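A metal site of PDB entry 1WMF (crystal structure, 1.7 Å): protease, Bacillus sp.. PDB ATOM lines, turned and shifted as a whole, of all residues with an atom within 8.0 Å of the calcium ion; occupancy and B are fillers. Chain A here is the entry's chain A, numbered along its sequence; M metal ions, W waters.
The backbone NH of Asn 390 sits close to the side-chain carboxylate of Asp 384.
The calcium ion is bound by OD1 of Asn 392.
The calcium ion is bound by OD1 of Asp 391, 2.3 Å away.
O of Thr 386 is bound to the calcium ion (2.4 Å).
OD1 of Asp 384 binds the calcium ion (2.4 Å).
The calcium ion is bound by water W1 (2.4 Å).
The calcium ion is bound by the backbone carbonyl oxygen (O) of Pro 388 (2.4 Å).
The calcium ion is bound by OD2 of Asp 384 (2.5 Å).
The calcium ion is bound by OG1 of Thr 386.
The calcium ion has eight donor atoms within binding distance.
Water W1 bridges the side-chain carboxylate of Asp 391 (2.9 Å) and the backbone carbonyl oxygen of Ser 387 (3.5 Å).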
ATOM      1  N   VAL A 381      -5.391  18.284  24.110  1.00  0.00           N
ATOM      2  CA  VAL A 381      -4.304  18.802  23.294  1.00  0.00           C
ATOM      3  C   VAL A 381      -3.246  19.404  24.205  1.00  0.00           C
ATOM      4  O   VAL A 381      -3.613  20.057  25.176  1.00  0.00           O
ATOM      5  CB  VAL A 381      -4.916  19.821  22.317  1.00  0.00           C
ATOM      6  CG1 VAL A 381      -3.879  20.737  21.718  1.00  0.00           C
ATOM      7  CG2 VAL A 381      -5.689  19.049  21.250  1.00  0.00           C
ATOM      8  N   ASN A 383      -0.936  21.516  26.323  1.00  0.00           N
ATOM      9  CA  ASN A 383      -0.971  22.844  26.898  1.00  0.00           C
ATOM     10  C   ASN A 383      -2.320  23.552  26.760  1.00  0.00           C
ATOM     11  O   ASN A 383      -2.429  24.756  26.973  1.00  0.00           O
ATOM     12  CB  ASN A 383       0.131  23.751  26.316  1.00  0.00           C
ATOM     13  CG  ASN A 383       1.513  23.228  26.687  1.00  0.00           C
ATOM     14  OD1 ASN A 383       1.659  22.404  27.595  1.00  0.00           O
ATOM     15  ND2 ASN A 383       2.562  23.692  26.009  1.00  0.00           N
ATOM     16  N   ASP A 384      -3.387  22.830  26.427  1.00  0.00           N
ATOM     17  CA  ASP A 384      -4.720  23.417  26.430  1.00  0.00           C
ATOM     18  C   ASP A 384      -5.377  23.208  27.804  1.00  0.00           C
ATOM     19  O   ASP A 384      -5.856  22.104  28.095  1.00  0.00           O
ATOM     20  CB  ASP A 384      -5.628  22.835  25.346  1.00  0.00           C
ATOM     21  CG  ASP A 384      -6.928  23.618  25.204  1.00  0.00           C
ATOM     22  OD1 ASP A 384      -7.250  24.409  26.115  1.00  0.00           O
ATOM     23  OD2 ASP A 384      -7.695  23.322  24.277  1.00  0.00           O
ATOM     24  N   PHE A 385      -5.383  24.278  28.599  1.00  0.00           N
ATOM     25  CA  PHE A 385      -5.926  24.207  29.950  1.00  0.00           C
ATOM     26  C   PHE A 385      -7.298  24.854  30.068  1.00  0.00           C
ATOM     27  O   PHE A 385      -7.784  25.091  31.186  1.00  0.00           O
ATOM     28  CB  PHE A 385      -4.932  24.844  30.928  1.00  0.00           C
ATOM     29  CG  PHE A 385      -3.681  23.995  31.116  1.00  0.00           C
ATOM     30  CD1 PHE A 385      -2.548  24.201  30.348  1.00  0.00           C
ATOM     31  CD2 PHE A 385      -3.654  22.983  32.055  1.00  0.00           C
ATOM     32  CE1 PHE A 385      -1.418  23.419  30.516  1.00  0.00           C
ATOM     33  CE2 PHE A 385      -2.540  22.192  32.246  1.00  0.00           C
ATOM     34  CZ  PHE A 385      -1.412  22.410  31.450  1.00  0.00           C
ATOM     35  N   THR A 386      -7.950  25.130  28.937  1.00  0.00           N
ATOM     36  CA  THR A 386      -9.306  25.677  28.993  1.00  0.00           C
ATOM     37  C   THR A 386     -10.299  24.718  28.379  1.00  0.00           C
ATOM     38  O   THR A 386     -10.054  24.229  27.282  1.00  0.00           O
ATOM     39  CB  THR A 386      -9.405  26.993  28.217  1.00  0.00           C
ATOM     40  OG1 THR A 386      -8.948  26.762  26.871  1.00  0.00           O
ATOM     41  CG2 THR A 386      -8.524  28.025  28.892  1.00  0.00           C
ATOM     42  N   SER A 387     -11.406  24.442  29.064  1.00  0.00           N
ATOM     43  CA  SER A 387     -12.391  23.532  28.462  1.00  0.00           C
ATOM     44  C   SER A 387     -13.053  24.185  27.271  1.00  0.00           C
ATOM     45  O   SER A 387     -13.364  25.380  27.413  1.00  0.00           O
ATOM     46  CB  SER A 387     -13.460  23.133  29.479  1.00  0.00           C
ATOM     47  OG  SER A 387     -14.276  22.105  28.955  1.00  0.00           O
ATOM     48  N   PRO A 388     -13.328  23.564  26.132  1.00  0.00           N
ATOM     49  CA  PRO A 388     -12.940  22.199  25.775  1.00  0.00           C
ATOM     50  C   PRO A 388     -11.423  22.083  25.566  1.00  0.00           C
ATOM     51  O   PRO A 388     -10.829  23.005  25.011  1.00  0.00           O
ATOM     52  CB  PRO A 388     -13.638  21.957  24.438  1.00  0.00           C
ATOM     53  CG  PRO A 388     -14.455  23.150  24.113  1.00  0.00           C
ATOM     54  CD  PRO A 388     -14.120  24.247  25.083  1.00  0.00           C
ATOM     55  N   TYR A 389     -10.809  20.989  26.035  1.00  0.00           N
ATOM     56  CA  TYR A 389      -9.362  20.909  26.089  1.00  0.00           C
ATOM     57  C   TYR A 389      -8.690  20.486  24.794  1.00  0.00           C
ATOM     58  O   TYR A 389      -7.509  20.128  24.822  1.00  0.00           O
ATOM     59  CB  TYR A 389      -8.936  19.889  27.158  1.00  0.00           C
ATOM     60  CG  TYR A 389      -9.470  20.352  28.498  1.00  0.00           C
ATOM     61  CD1 TYR A 389     -10.447  19.608  29.139  1.00  0.00           C
ATOM     62  CD2 TYR A 389      -9.015  21.535  29.081  1.00  0.00           C
ATOM     63  CE1 TYR A 389     -10.964  20.005  30.358  1.00  0.00           C
ATOM     64  CE2 TYR A 389      -9.528  21.941  30.310  1.00  0.00           C
ATOM     65  CZ  TYR A 389     -10.502  21.177  30.928  1.00  0.00           C
ATOM     66  OH  TYR A 389     -11.032  21.556  32.148  1.00  0.00           O
ATOM     67  N   ASN A 390      -9.444  20.520  23.706  1.00  0.00           N
ATOM     68  CA  ASN A 390      -8.907  20.053  22.426  1.00  0.00           C
ATOM     69  C   ASN A 390      -9.046  21.108  21.331  1.00  0.00           C
ATOM     70  O   ASN A 390      -9.042  20.745  20.152  1.00  0.00           O
ATOM     71  CB  ASN A 390      -9.574  18.739  21.981  1.00  0.00           C
ATOM     72  CG  ASN A 390     -11.022  18.837  21.590  1.00  0.00           C
ATOM     73  OD1 ASN A 390     -11.715  19.820  21.888  1.00  0.00           O
ATOM     74  ND2 ASN A 390     -11.571  17.833  20.908  1.00  0.00           N
ATOM     75  N   ASP A 391      -9.169  22.388  21.675  1.00  0.00           N
ATOM     76  CA  ASP A 391      -9.395  23.362  20.601  1.00  0.00           C
ATOM     77  C   ASP A 391      -8.274  24.383  20.506  1.00  0.00           C
ATOM     78  O   ASP A 391      -8.253  25.186  19.571  1.00  0.00           O
ATOM     79  CB  ASP A 391     -10.741  24.065  20.760  1.00  0.00           C
ATOM     80  CG  ASP A 391     -10.933  24.758  22.077  1.00  0.00           C
ATOM     81  OD1 ASP A 391      -9.956  24.780  22.886  1.00  0.00           O
ATOM     82  OD2 ASP A 391     -12.051  25.276  22.294  1.00  0.00           O
ATOM     83  N   ASN A 392      -7.346  24.364  21.445  1.00  0.00           N
ATOM     84  CA  ASN A 392      -6.239  25.312  21.419  1.00  0.00           C
ATOM     85  C   ASN A 392      -4.909  24.574  21.210  1.00  0.00           C
ATOM     86  O   ASN A 392      -4.377  23.952  22.123  1.00  0.00           O
ATOM     87  CB  ASN A 392      -6.175  26.104  22.720  1.00  0.00           C
ATOM     88  CG  ASN A 392      -7.419  26.871  23.118  1.00  0.00           C
ATOM     89  OD1 ASN A 392      -8.047  26.546  24.128  1.00  0.00           O
ATOM     90  ND2 ASN A 392      -7.761  27.885  22.339  1.00  0.00           N
ATOM     91  N   TRP A 393      -4.367  24.627  20.001  1.00  0.00           N
ATOM     92  CA  TRP A 393      -3.110  23.964  19.701  1.00  0.00           C
ATOM     93  C   TRP A 393      -1.877  24.799  19.977  1.00  0.00           C
ATOM     94  O   TRP A 393      -1.890  26.029  19.863  1.00  0.00           O
ATOM     95  CB  TRP A 393      -3.105  23.557  18.221  1.00  0.00           C
ATOM     96  CG  TRP A 393      -4.233  22.585  17.983  1.00  0.00           C
ATOM     97  CD1 TRP A 393      -5.558  22.865  17.857  1.00  0.00           C
ATOM     98  CD2 TRP A 393      -4.071  21.178  17.836  1.00  0.00           C
ATOM     99  NE1 TRP A 393      -6.257  21.695  17.656  1.00  0.00           N
ATOM    100  CE2 TRP A 393      -5.354  20.649  17.636  1.00  0.00           C
ATOM    101  CE3 TRP A 393      -2.972  20.317  17.861  1.00  0.00           C
ATOM    102  CZ2 TRP A 393      -5.547  19.280  17.454  1.00  0.00           C
ATOM    103  CZ3 TRP A 393      -3.170  18.958  17.692  1.00  0.00           C
ATOM    104  CH2 TRP A 393      -4.453  18.449  17.483  1.00  0.00           C
HETATM  105 CA    CA M   1      -9.362  24.948  25.142  1.00  0.00          CA
HETATM  106  O   HOH W   1     -11.250  26.430  24.862  1.00  0.00           O
